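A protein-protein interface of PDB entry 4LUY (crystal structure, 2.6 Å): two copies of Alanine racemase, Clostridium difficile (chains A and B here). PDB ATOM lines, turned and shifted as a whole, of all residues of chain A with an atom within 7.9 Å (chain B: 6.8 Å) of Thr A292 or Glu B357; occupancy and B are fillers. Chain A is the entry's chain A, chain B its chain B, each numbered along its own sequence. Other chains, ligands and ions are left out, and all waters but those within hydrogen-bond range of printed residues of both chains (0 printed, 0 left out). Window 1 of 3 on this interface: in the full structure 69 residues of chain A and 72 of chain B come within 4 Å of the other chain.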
ATOM      1  N   LEU A 250      34.598 -13.740   4.529  1.00  0.00           N
ATOM      2  CA  LEU A 250      33.913 -14.985   4.582  1.00  0.00           C
ATOM      3  C   LEU A 250      33.350 -15.204   3.220  1.00  0.00           C
ATOM      4  O   LEU A 250      32.563 -14.449   2.769  1.00  0.00           O
ATOM      5  CB  LEU A 250      32.785 -14.925   5.591  1.00  0.00           C
ATOM      6  CG  LEU A 250      32.080 -16.198   6.031  1.00  0.00           C
ATOM      7  CD1 LEU A 250      33.086 -17.240   6.379  1.00  0.00           C
ATOM      8  CD2 LEU A 250      31.197 -15.994   7.201  1.00  0.00           C
ATOM      9  N   ILE A 285      26.700 -22.284   3.132  1.00  0.00           N
ATOM     10  CA  ILE A 285      27.055 -21.848   4.413  1.00  0.00           C
ATOM     11  C   ILE A 285      25.777 -21.802   5.226  1.00  0.00           C
ATOM     12  O   ILE A 285      24.747 -21.557   4.720  1.00  0.00           O
ATOM     13  CB  ILE A 285      27.731 -20.499   4.386  1.00  0.00           C
ATOM     14  CG1 ILE A 285      28.253 -20.166   5.759  1.00  0.00           C
ATOM     15  CG2 ILE A 285      26.758 -19.435   3.968  1.00  0.00           C
ATOM     16  CD1 ILE A 285      29.157 -18.975   5.810  1.00  0.00           C
ATOM     17  N   GLY A 286      25.905 -22.022   6.509  1.00  0.00           N
ATOM     18  CA  GLY A 286      24.831 -21.974   7.453  1.00  0.00           C
ATOM     19  C   GLY A 286      25.327 -21.575   8.819  1.00  0.00           C
ATOM     20  O   GLY A 286      26.417 -21.177   8.964  1.00  0.00           O
ATOM     21  N   TYR A 287      24.496 -21.701   9.829  1.00  0.00           N
ATOM     22  CA  TYR A 287      24.803 -21.307  11.187  1.00  0.00           C
ATOM     23  C   TYR A 287      25.896 -22.048  11.907  1.00  0.00           C
ATOM     24  O   TYR A 287      26.533 -21.514  12.750  1.00  0.00           O
ATOM     25  CB  TYR A 287      23.576 -21.152  12.056  1.00  0.00           C
ATOM     26  CG  TYR A 287      22.793 -22.376  12.331  1.00  0.00           C
ATOM     27  CD1 TYR A 287      23.257 -23.343  13.175  1.00  0.00           C
ATOM     28  CD2 TYR A 287      21.574 -22.556  11.778  1.00  0.00           C
ATOM     29  CE1 TYR A 287      22.547 -24.453  13.416  1.00  0.00           C
ATOM     30  CE2 TYR A 287      20.861 -23.661  12.033  1.00  0.00           C
ATOM     31  CZ  TYR A 287      21.359 -24.598  12.846  1.00  0.00           C
ATOM     32  OH  TYR A 287      20.627 -25.678  13.079  1.00  0.00           O
ATOM     33  N   ALA A 288      26.117 -23.279  11.521  1.00  0.00           N
ATOM     34  CA  ALA A 288      27.183 -24.064  12.048  1.00  0.00           C
ATOM     35  C   ALA A 288      28.534 -23.702  11.461  1.00  0.00           C
ATOM     36  O   ALA A 288      29.522 -24.223  11.832  1.00  0.00           O
ATOM     37  CB  ALA A 288      26.886 -25.521  11.911  1.00  0.00           C
ATOM     38  N   ASP A 289      28.553 -22.787  10.541  1.00  0.00           N
ATOM     39  CA  ASP A 289      29.765 -22.153  10.118  1.00  0.00           C
ATOM     40  C   ASP A 289      29.989 -20.856  10.840  1.00  0.00           C
ATOM     41  O   ASP A 289      30.982 -20.246  10.743  1.00  0.00           O
ATOM     42  CB  ASP A 289      29.731 -21.939   8.615  1.00  0.00           C
ATOM     43  CG  ASP A 289      29.623 -23.205   7.851  1.00  0.00           C
ATOM     44  OD1 ASP A 289      30.550 -23.952   7.783  1.00  0.00           O
ATOM     45  OD2 ASP A 289      28.594 -23.482   7.324  1.00  0.00           O
ATOM     46  N   GLY A 290      29.010 -20.493  11.608  1.00  0.00           N
ATOM     47  CA  GLY A 290      28.975 -19.227  12.248  1.00  0.00           C
ATOM     48  C   GLY A 290      28.220 -18.147  11.575  1.00  0.00           C
ATOM     49  O   GLY A 290      28.305 -17.046  11.987  1.00  0.00           O
ATOM     50  N   PHE A 291      27.502 -18.463  10.527  1.00  0.00           N
ATOM     51  CA  PHE A 291      26.630 -17.506   9.914  1.00  0.00           C
ATOM     52  C   PHE A 291      25.322 -17.603  10.619  1.00  0.00           C
ATOM     53  O   PHE A 291      24.440 -18.218  10.181  1.00  0.00           O
ATOM     54  CB  PHE A 291      26.474 -17.772   8.431  1.00  0.00           C
ATOM     55  CG  PHE A 291      25.963 -16.612   7.667  1.00  0.00           C
ATOM     56  CD1 PHE A 291      26.628 -15.446   7.654  1.00  0.00           C
ATOM     57  CD2 PHE A 291      24.800 -16.690   6.994  1.00  0.00           C
ATOM     58  CE1 PHE A 291      26.149 -14.382   6.977  1.00  0.00           C
ATOM     59  CE2 PHE A 291      24.306 -15.641   6.330  1.00  0.00           C
ATOM     60  CZ  PHE A 291      24.984 -14.482   6.317  1.00  0.00           C
ATOM     61  N   THR A 292      25.213 -16.951  11.734  1.00  0.00           N
ATOM     62  CA  THR A 292      24.193 -17.240  12.673  1.00  0.00           C
ATOM     63  C   THR A 292      22.780 -17.054  12.217  1.00  0.00           C
ATOM     64  O   THR A 292      22.468 -16.123  11.565  1.00  0.00           O
ATOM     65  CB  THR A 292      24.430 -16.488  13.979  1.00  0.00           C
ATOM     66  OG1 THR A 292      23.430 -16.833  14.884  1.00  0.00           O
ATOM     67  CG2 THR A 292      24.374 -15.082  13.809  1.00  0.00           C
ATOM     68  N   ARG A 293      21.947 -17.980  12.636  1.00  0.00           N
ATOM     69  CA  ARG A 293      20.530 -18.010  12.440  1.00  0.00           C
ATOM     70  C   ARG A 293      19.828 -16.835  13.085  1.00  0.00           C
ATOM     71  O   ARG A 293      18.762 -16.469  12.723  1.00  0.00           O
ATOM     72  CB  ARG A 293      20.014 -19.281  13.050  1.00  0.00           C
ATOM     73  CG  ARG A 293      18.686 -19.722  12.564  1.00  0.00           C
ATOM     74  CD  ARG A 293      18.269 -20.912  13.313  1.00  0.00           C
ATOM     75  NE  ARG A 293      17.005 -21.444  12.871  1.00  0.00           N
ATOM     76  CZ  ARG A 293      15.865 -21.177  13.457  1.00  0.00           C
ATOM     77  NH1 ARG A 293      15.829 -20.364  14.470  1.00  0.00           N
ATOM     78  NH2 ARG A 293      14.781 -21.714  13.020  1.00  0.00           N
ATOM     79  N   ILE A 294      20.477 -16.246  14.041  1.00  0.00           N
ATOM     80  CA  ILE A 294      19.924 -15.177  14.792  1.00  0.00           C
ATOM     81  C   ILE A 294      19.666 -13.946  13.960  1.00  0.00           C
ATOM     82  O   ILE A 294      18.864 -13.151  14.315  1.00  0.00           O
ATOM     83  CB  ILE A 294      20.699 -14.959  16.114  1.00  0.00           C
ATOM     84  CG1 ILE A 294      20.459 -16.163  16.996  1.00  0.00           C
ATOM     85  CG2 ILE A 294      20.202 -13.756  16.876  1.00  0.00           C
ATOM     86  CD1 ILE A 294      21.579 -16.539  17.876  1.00  0.00           C
ATOM     87  N   GLN A 295      20.322 -13.822  12.830  1.00  0.00           N
ATOM     88  CA  GLN A 295      20.209 -12.646  12.000  1.00  0.00           C
ATOM     89  C   GLN A 295      18.820 -12.367  11.442  1.00  0.00           C
ATOM     90  O   GLN A 295      18.213 -13.207  10.854  1.00  0.00           O
ATOM     91  CB  GLN A 295      21.147 -12.787  10.844  1.00  0.00           C
ATOM     92  CG  GLN A 295      22.576 -12.520  11.141  1.00  0.00           C
ATOM     93  CD  GLN A 295      23.423 -12.776   9.954  1.00  0.00           C
ATOM     94  OE1 GLN A 295      23.774 -11.884   9.252  1.00  0.00           O
ATOM     95  NE2 GLN A 295      23.732 -13.988   9.727  1.00  0.00           N
ATOM     96  N   LYS A 296      18.305 -11.196  11.722  1.00  0.00           N
ATOM     97  CA  LYS A 296      17.063 -10.760  11.177  1.00  0.00           C
ATOM     98  C   LYS A 296      17.042 -10.385   9.719  1.00  0.00           C
ATOM     99  O   LYS A 296      16.074 -10.612   9.044  1.00  0.00           O
ATOM    100  CB  LYS A 296      16.385  -9.747  12.065  1.00  0.00           C
ATOM    101  CG  LYS A 296      15.803 -10.368  13.309  1.00  0.00           C
ATOM    102  CD  LYS A 296      15.864  -9.423  14.473  1.00  0.00           C
ATOM    103  CE  LYS A 296      15.094  -9.935  15.649  1.00  0.00           C
ATOM    104  NZ  LYS A 296      14.812  -8.908  16.659  1.00  0.00           N
ATOM    105  N   PRO A 298      19.669 -11.009   7.057  1.00  0.00           N
ATOM    106  CA  PRO A 298      20.910 -11.495   6.487  1.00  0.00           C
ATOM    107  C   PRO A 298      21.123 -11.074   5.069  1.00  0.00           C
ATOM    108  O   PRO A 298      20.198 -11.095   4.337  1.00  0.00           O
ATOM    109  CB  PRO A 298      20.721 -12.995   6.519  1.00  0.00           C
ATOM    110  CG  PRO A 298      19.648 -13.235   7.453  1.00  0.00           C
ATOM    111  CD  PRO A 298      18.738 -12.106   7.255  1.00  0.00           C
ATOM    112  N   ILE A 313      17.806 -19.626   8.197  1.00  0.00           N
ATOM    113  CA  ILE A 313      19.099 -20.203   7.930  1.00  0.00           C
ATOM    114  C   ILE A 313      19.172 -21.630   8.469  1.00  0.00           C
ATOM    115  O   ILE A 313      18.677 -21.947   9.502  1.00  0.00           O
ATOM    116  CB  ILE A 313      20.181 -19.300   8.518  1.00  0.00           C
ATOM    117  CG1 ILE A 313      20.227 -17.980   7.787  1.00  0.00           C
ATOM    118  CG2 ILE A 313      21.553 -19.920   8.513  1.00  0.00           C
ATOM    119  CD1 ILE A 313      21.285 -17.064   8.306  1.00  0.00           C
ATOM    120  N   CYS A 314      19.732 -22.506   7.689  1.00  0.00           N
ATOM    121  CA  CYS A 314      19.971 -23.854   8.102  1.00  0.00           C
ATOM    122  C   CYS A 314      21.364 -24.033   8.609  1.00  0.00           C
ATOM    123  O   CYS A 314      22.135 -23.158   8.614  1.00  0.00           O
ATOM    124  CB  CYS A 314      19.681 -24.807   6.965  1.00  0.00           C
ATOM    125  SG  CYS A 314      18.074 -24.581   6.305  1.00  0.00           S
ATOM    126  N   MET A 315      21.651 -25.212   9.056  1.00  0.00           N
ATOM    127  CA  MET A 315      22.863 -25.518   9.730  1.00  0.00           C
ATOM    128  C   MET A 315      24.029 -25.307   8.816  1.00  0.00           C
ATOM    129  O   MET A 315      25.048 -24.851   9.202  1.00  0.00           O
ATOM    130  CB  MET A 315      22.792 -26.964  10.180  1.00  0.00           C
ATOM    131  CG  MET A 315      23.691 -27.374  11.333  1.00  0.00           C
ATOM    132  SD  MET A 315      23.630 -29.085  11.743  1.00  0.00           S
ATOM    133  CE  MET A 315      22.546 -29.058  13.100  1.00  0.00           C
ATOM    134  N   ILE A 318      21.883 -21.888   3.080  1.00  0.00           N
ATOM    135  CA  ILE A 318      21.006 -20.736   2.972  1.00  0.00           C
ATOM    136  C   ILE A 318      20.462 -20.575   1.600  1.00  0.00           C
ATOM    137  O   ILE A 318      21.022 -21.038   0.660  1.00  0.00           O
ATOM    138  CB  ILE A 318      21.664 -19.395   3.245  1.00  0.00           C
ATOM    139  CG1 ILE A 318      23.082 -19.370   2.781  1.00  0.00           C
ATOM    140  CG2 ILE A 318      21.616 -19.041   4.687  1.00  0.00           C
ATOM    141  CD1 ILE A 318      23.626 -17.987   2.798  1.00  0.00           C
ATOM    142  N   ILE A 347      26.553  -6.940  10.241  1.00  0.00           N
ATOM    143  CA  ILE A 347      26.039  -8.147  10.789  1.00  0.00           C
ATOM    144  C   ILE A 347      25.952  -7.967  12.257  1.00  0.00           C
ATOM    145  O   ILE A 347      25.026  -8.373  12.843  1.00  0.00           O
ATOM    146  CB  ILE A 347      26.921  -9.343  10.427  1.00  0.00           C
ATOM    147  CG1 ILE A 347      26.822  -9.648   8.964  1.00  0.00           C
ATOM    148  CG2 ILE A 347      26.482 -10.579  11.147  1.00  0.00           C
ATOM    149  CD1 ILE A 347      27.818 -10.622   8.463  1.00  0.00           C
ATOM    150  N   ASP A 350      23.012  -5.689  13.275  1.00  0.00           N
ATOM    151  CA  ASP A 350      21.803  -6.447  13.130  1.00  0.00           C
ATOM    152  C   ASP A 350      21.623  -7.403  14.277  1.00  0.00           C
ATOM    153  O   ASP A 350      20.557  -7.545  14.804  1.00  0.00           O
ATOM    154  CB  ASP A 350      21.838  -7.201  11.810  1.00  0.00           C
ATOM    155  CG  ASP A 350      20.567  -7.899  11.492  1.00  0.00           C
ATOM    156  OD1 ASP A 350      19.533  -7.317  11.724  1.00  0.00           O
ATOM    157  OD2 ASP A 350      20.582  -8.998  10.975  1.00  0.00           O
ATOM    158  N   LEU A 351      22.676  -8.090  14.618  1.00  0.00           N
ATOM    159  CA  LEU A 351      22.649  -8.998  15.704  1.00  0.00           C
ATOM    160  C   LEU A 351      22.448  -8.327  17.017  1.00  0.00           C
ATOM    161  O   LEU A 351      21.875  -8.889  17.892  1.00  0.00           O
ATOM    162  CB  LEU A 351      23.886  -9.837  15.722  1.00  0.00           C
ATOM    163  CG  LEU A 351      23.919 -11.239  15.182  1.00  0.00           C
ATOM    164  CD1 LEU A 351      22.635 -11.765  14.666  1.00  0.00           C
ATOM    165  CD2 LEU A 351      25.014 -11.371  14.192  1.00  0.00           C
ATOM    166  N   THR A 353      25.322  -7.103  18.493  1.00  0.00           N
ATOM    167  CA  THR A 353      26.615  -7.368  19.052  1.00  0.00           C
ATOM    168  C   THR A 353      27.691  -6.510  18.436  1.00  0.00           C
ATOM    169  O   THR A 353      27.421  -5.491  17.900  1.00  0.00           O
ATOM    170  CB  THR A 353      26.949  -8.856  19.060  1.00  0.00           C
ATOM    171  OG1 THR A 353      28.119  -9.076  19.815  1.00  0.00           O
ATOM    172  CG2 THR A 353      27.149  -9.362  17.733  1.00  0.00           C
ATOM    173  N   GLU A 357      32.685 -10.338  18.123  1.00  0.00           N
ATOM    174  CA  GLU A 357      32.025 -11.610  18.138  1.00  0.00           C
ATOM    175  C   GLU A 357      31.784 -12.258  16.800  1.00  0.00           C
ATOM    176  O   GLU A 357      31.883 -13.429  16.683  1.00  0.00           O
ATOM    177  CB  GLU A 357      30.768 -11.581  18.972  1.00  0.00           C
ATOM    178  CG  GLU A 357      30.046 -12.886  18.973  1.00  0.00           C
ATOM    179  CD  GLU A 357      28.894 -12.914  19.871  1.00  0.00           C
ATOM    180  OE1 GLU A 357      28.311 -11.896  20.065  1.00  0.00           O
ATOM    181  OE2 GLU A 357      28.567 -13.955  20.361  1.00  0.00           O
ATOM    182  N   VAL A 358      31.468 -11.477  15.796  1.00  0.00           N
ATOM    183  CA  VAL A 358      31.278 -11.997  14.485  1.00  0.00           C
ATOM    184  C   VAL A 358      32.551 -12.621  13.946  1.00  0.00           C
ATOM    185  O   VAL A 358      32.503 -13.641  13.348  1.00  0.00           O
ATOM    186  CB  VAL A 358      30.786 -10.903  13.536  1.00  0.00           C
ATOM    187  CG1 VAL A 358      30.742 -11.384  12.123  1.00  0.00           C
ATOM    188  CG2 VAL A 358      29.432 -10.406  13.930  1.00  0.00           C
ATOM    189  N   MET A 361      33.042 -16.032  15.440  1.00  0.00           N
ATOM    190  CA  MET A 361      32.027 -17.033  15.202  1.00  0.00           C
ATOM    191  C   MET A 361      32.311 -18.062  14.146  1.00  0.00           C
ATOM    192  O   MET A 361      31.625 -19.018  14.068  1.00  0.00           O
ATOM    193  CB  MET A 361      30.703 -16.404  14.897  1.00  0.00           C
ATOM    194  CG  MET A 361      29.892 -16.036  16.095  1.00  0.00           C
ATOM    195  SD  MET A 361      28.444 -15.149  15.676  1.00  0.00           S
ATOM    196  CE  MET A 361      27.513 -15.057  17.133  1.00  0.00           C
ATOM    197  N   ILE B 294      25.083 -12.286  22.745  1.00  0.00           N
ATOM    198  CA  ILE B 294      23.774 -11.861  22.410  1.00  0.00           C
ATOM    199  C   ILE B 294      22.749 -12.193  23.444  1.00  0.00           C
ATOM    200  O   ILE B 294      21.661 -11.759  23.345  1.00  0.00           O
ATOM    201  CB  ILE B 294      23.356 -12.420  21.065  1.00  0.00           C
ATOM    202  CG1 ILE B 294      24.389 -12.099  20.041  1.00  0.00           C
ATOM    203  CG2 ILE B 294      22.080 -11.814  20.600  1.00  0.00           C
ATOM    204  CD1 ILE B 294      24.065 -12.645  18.699  1.00  0.00           C
ATOM    205  N   ALA B 348      18.519 -21.008  23.954  1.00  0.00           N
ATOM    206  CA  ALA B 348      18.014 -20.823  22.636  1.00  0.00           C
ATOM    207  C   ALA B 348      16.794 -19.951  22.545  1.00  0.00           C
ATOM    208  O   ALA B 348      16.643 -19.231  21.611  1.00  0.00           O
ATOM    209  CB  ALA B 348      17.753 -22.152  22.004  1.00  0.00           C
ATOM    210  N   LEU B 351      17.717 -16.416  23.034  1.00  0.00           N
ATOM    211  CA  LEU B 351      18.252 -16.019  21.769  1.00  0.00           C
ATOM    212  C   LEU B 351      17.251 -15.862  20.675  1.00  0.00           C
ATOM    213  O   LEU B 351      17.415 -15.055  19.815  1.00  0.00           O
ATOM    214  CB  LEU B 351      19.345 -16.959  21.374  1.00  0.00           C
ATOM    215  CG  LEU B 351      20.792 -16.695  21.651  1.00  0.00           C
ATOM    216  CD1 LEU B 351      21.112 -15.640  22.633  1.00  0.00           C
ATOM    217  CD2 LEU B 351      21.396 -17.960  22.084  1.00  0.00           C
ATOM    218  N   GLY B 352      16.207 -16.645  20.709  1.00  0.00           N
ATOM    219  CA  GLY B 352      15.291 -16.688  19.625  1.00  0.00           C
ATOM    220  C   GLY B 352      15.734 -17.552  18.504  1.00  0.00           C
ATOM    221  O   GLY B 352      15.374 -17.318  17.403  1.00  0.00           O
ATOM    222  N   THR B 353      16.550 -18.532  18.824  1.00  0.00           N
ATOM    223  CA  THR B 353      17.027 -19.523  17.903  1.00  0.00           C
ATOM    224  C   THR B 353      16.610 -20.898  18.362  1.00  0.00           C
ATOM    225  O   THR B 353      15.776 -21.008  19.157  1.00  0.00           O
ATOM    226  CB  THR B 353      18.525 -19.401  17.669  1.00  0.00           C
ATOM    227  OG1 THR B 353      18.921 -20.309  16.666  1.00  0.00           O
ATOM    228  CG2 THR B 353      19.285 -19.674  18.892  1.00  0.00           C
ATOM    229  N   ILE B 354      17.209 -21.934  17.856  1.00  0.00           N
ATOM    230  CA  ILE B 354      16.830 -23.276  18.189  1.00  0.00           C
ATOM    231  C   ILE B 354      17.966 -24.035  18.804  1.00  0.00           C
ATOM    232  O   ILE B 354      19.072 -23.696  18.631  1.00  0.00           O
ATOM    233  CB  ILE B 354      16.384 -24.041  16.970  1.00  0.00           C
ATOM    234  CG1 ILE B 354      17.364 -23.879  15.866  1.00  0.00           C
ATOM    235  CG2 ILE B 354      15.081 -23.520  16.481  1.00  0.00           C
ATOM    236  CD1 ILE B 354      17.090 -24.752  14.705  1.00  0.00           C
ATOM    237  N   ASN B 355      17.671 -25.098  19.495  1.00  0.00           N
ATOM    238  CA  ASN B 355      18.655 -25.768  20.296  1.00  0.00           C
ATOM    239  C   ASN B 355      19.786 -26.264  19.470  1.00  0.00           C
ATOM    240  O   ASN B 355      20.865 -26.414  19.949  1.00  0.00           O
ATOM    241  CB  ASN B 355      18.036 -26.905  21.111  1.00  0.00           C
ATOM    242  CG  ASN B 355      17.120 -27.788  20.300  1.00  0.00           C
ATOM    243  OD1 ASN B 355      17.017 -27.646  19.133  1.00  0.00           O
ATOM    244  ND2 ASN B 355      16.476 -28.709  20.936  1.00  0.00           N
ATOM    245  N   TYR B 356      19.497 -26.510  18.207  1.00  0.00           N
ATOM    246  CA  TYR B 356      20.440 -27.012  17.263  1.00  0.00           C
ATOM    247  C   TYR B 356      21.569 -26.043  17.104  1.00  0.00           C
ATOM    248  O   TYR B 356      22.644 -26.442  16.956  1.00  0.00           O
ATOM    249  CB  TYR B 356      19.811 -27.131  15.901  1.00  0.00           C
ATOM    250  CG  TYR B 356      18.735 -28.137  15.610  1.00  0.00           C
ATOM    251  CD1 TYR B 356      17.463 -27.959  16.033  1.00  0.00           C
ATOM    252  CD2 TYR B 356      18.981 -29.201  14.808  1.00  0.00           C
ATOM    253  CE1 TYR B 356      16.483 -28.854  15.726  1.00  0.00           C
ATOM    254  CE2 TYR B 356      18.009 -30.086  14.489  1.00  0.00           C
ATOM    255  CZ  TYR B 356      16.746 -29.893  14.942  1.00  0.00           C
ATOM    256  OH  TYR B 356      15.788 -30.755  14.590  1.00  0.00           O
ATOM    257  N   GLU B 357      21.280 -24.759  17.066  1.00  0.00           N
ATOM    258  CA  GLU B 357      22.316 -23.762  16.942  1.00  0.00           C
ATOM    259  C   GLU B 357      23.252 -23.638  18.123  1.00  0.00           C
ATOM    260  O   GLU B 357      24.406 -23.544  17.948  1.00  0.00           O
ATOM    261  CB  GLU B 357      21.777 -22.415  16.509  1.00  0.00           C
ATOM    262  CG  GLU B 357      22.860 -21.410  16.252  1.00  0.00           C
ATOM    263  CD  GLU B 357      22.431 -20.087  15.730  1.00  0.00           C
ATOM    264  OE1 GLU B 357      21.359 -19.655  15.983  1.00  0.00           O
ATOM    265  OE2 GLU B 357      23.206 -19.442  15.095  1.00  0.00           O
ATOM    266  N   VAL B 358      22.704 -23.686  19.315  1.00  0.00           N
ATOM    267  CA  VAL B 358      23.414 -23.631  20.559  1.00  0.00           C
ATOM    268  C   VAL B 358      24.374 -24.789  20.782  1.00  0.00           C
ATOM    269  O   VAL B 358      25.411 -24.627  21.305  1.00  0.00           O
ATOM    270  CB  VAL B 358      22.411 -23.530  21.724  1.00  0.00           C
ATOM    271  CG1 VAL B 358      23.089 -23.508  23.034  1.00  0.00           C
ATOM    272  CG2 VAL B 358      21.592 -22.295  21.631  1.00  0.00           C
ATOM    273  N   LEU B 359      23.982 -25.968  20.387  1.00  0.00           N
ATOM    274  CA  LEU B 359      24.814 -27.116  20.398  1.00  0.00           C
ATOM    275  C   LEU B 359      25.966 -27.014  19.462  1.00  0.00           C
ATOM    276  O   LEU B 359      27.038 -27.413  19.749  1.00  0.00           O
ATOM    277  CB  LEU B 359      24.006 -28.309  20.015  1.00  0.00           C
ATOM    278  CG  LEU B 359      23.008 -28.817  21.021  1.00  0.00           C
ATOM    279  CD1 LEU B 359      22.353 -30.058  20.509  1.00  0.00           C
ATOM    280  CD2 LEU B 359      23.639 -29.082  22.355  1.00  0.00           C
ATOM    281  N   CYS B 360      25.685 -26.495  18.303  1.00  0.00           N
ATOM    282  CA  CYS B 360      26.652 -26.228  17.273  1.00  0.00           C
ATOM    283  C   CYS B 360      27.640 -25.128  17.550  1.00  0.00           C
ATOM    284  O   CYS B 360      28.655 -25.102  17.000  1.00  0.00           O
ATOM    285  CB  CYS B 360      25.944 -26.023  15.959  1.00  0.00           C
ATOM    286  SG  CYS B 360      25.485 -27.545  15.239  1.00  0.00           S
ATOM    287  N   MET B 361      27.283 -24.219  18.416  1.00  0.00           N
ATOM    288  CA  MET B 361      28.064 -23.062  18.755  1.00  0.00           C
ATOM    289  C   MET B 361      29.374 -23.293  19.466  1.00  0.00           C
ATOM    290  O   MET B 361      30.177 -22.421  19.477  1.00  0.00           O
ATOM    291  CB  MET B 361      27.266 -22.098  19.583  1.00  0.00           C
ATOM    292  CG  MET B 361      26.381 -21.210  18.787  1.00  0.00           C
ATOM    293  SD  MET B 361      25.456 -19.984  19.610  1.00  0.00           S
ATOM    294  CE  MET B 361      25.227 -18.856  18.327  1.00  0.00           C
ATOM    295  N   ILE B 362      29.547 -24.440  20.088  1.00  0.00           N
ATOM    296  CA  ILE B 362      30.722 -24.682  20.858  1.00  0.00           C
ATOM    297  C   ILE B 362      31.930 -24.603  19.977  1.00  0.00           C
ATOM    298  O   ILE B 362      32.022 -25.254  19.014  1.00  0.00           O
ATOM    299  CB  ILE B 362      30.655 -26.060  21.499  1.00  0.00           C
ATOM    300  CG1 ILE B 362      29.425 -26.188  22.340  1.00  0.00           C
ATOM    301  CG2 ILE B 362      31.807 -26.304  22.395  1.00  0.00           C
ATOM    302  CD1 ILE B 362      29.165 -25.032  23.237  1.00  0.00           C
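Of chain B, only Glu B357 comes within 4 Å of Thr A292. Of the printed residues of chain B, Arg A293 touches Thr B353 (3.5 Å), Ile B354 (3.8 Å) and Glu B357 (3.1 Å). Of the printed residues of chain B, Glu A357 touches Ile B294 (3.9 Å). Of chain A, only Tyr A287, Thr A292, Arg A293 and Ile A294 come within 4 Å of Glu B357. Printed residues of chain A within 4 Å of Cys B360: Met A315. The nearest printed residue of chain A that does not touch Ile B294 is Thr A353 (4.2 Å).
Ile A294 touches Leu B351, and with the chains exchanged Leu A351 touches Ile B294. Ile A294 touches Thr B353, but with the chains exchanged Thr A353 does not touch Ile B294 (4.2 Å). Ile A294 touches Glu B357, and with the chains exchanged Glu A357 touches Ile B294. Positions printed for both chains: 294, 351, 353, 357, 358 and 361. Of the 13 pairs that touch across the chains among the printed residues, 4 have their exchanged pair printed and touching as well.
Of the 25 printed residues of chain A, 7 touch a printed residue of chain B. Hydrophobic or aromatic side chains of chain A that line the printed part of chain B: Tyr A287, Ile A294, Met A315 and Leu A351. Along chain B the printed residues that touch a printed residue of chain A span positions 294 to 360. Among the printed residues, 13 pairs touch across the chains. Among the printed residues, no Asp or Glu carboxylate lies within 4 Å of a Lys or Arg side-chain nitrogen of the other chain.
Among the printed residues, pairs that only touch across the chains: Tyr A287 with Tyr B356, Tyr A287 with Glu B357, Arg A293 with Thr B353, Arg A293 with Ile B354, Ile A294 with Leu B351, Ile A294 with Thr B353, Ile A294 with Glu B357, Met A315 with Tyr B356, Met A315 with Cys B360, Leu A351 with Ile B294 and Glu A357 with Ile B294.
The side-chain hydroxyl (OG1) of Thr A292 is in hydrogen-bond range of the side-chain carboxylate (OE2) of Glu B357 (2.6 Å). N of Arg A293 sits at hydrogen-bond distance from OE2 of Glu B357 (3.1 Å).
OG1 of Thr B353 is in hydrogen-bond range of OE1 of Glu B357 (2.6 Å). N of Ala A288 lies within hydrogen-bond range of O of Met A315 (3.0 Å). The backbone NH (N) of Ile A294 lies close to the side-chain hydroxyl (OG1) of Thr A292, 3.1 Å away. The backbone carbonyl oxygen of Thr A292 sits at hydrogen-bond distance from the side-chain amide nitrogen of Gln A295, at 3.1 Å. The backbone NH (N) of Tyr A287 lies within hydrogen-bond range of the backbone carbonyl oxygen (O) of Met A315. The side-chain hydroxyl (OG1) of Thr A353 sits at hydrogen-bond distance from the side-chain carboxylate (OE1) of Glu A357.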
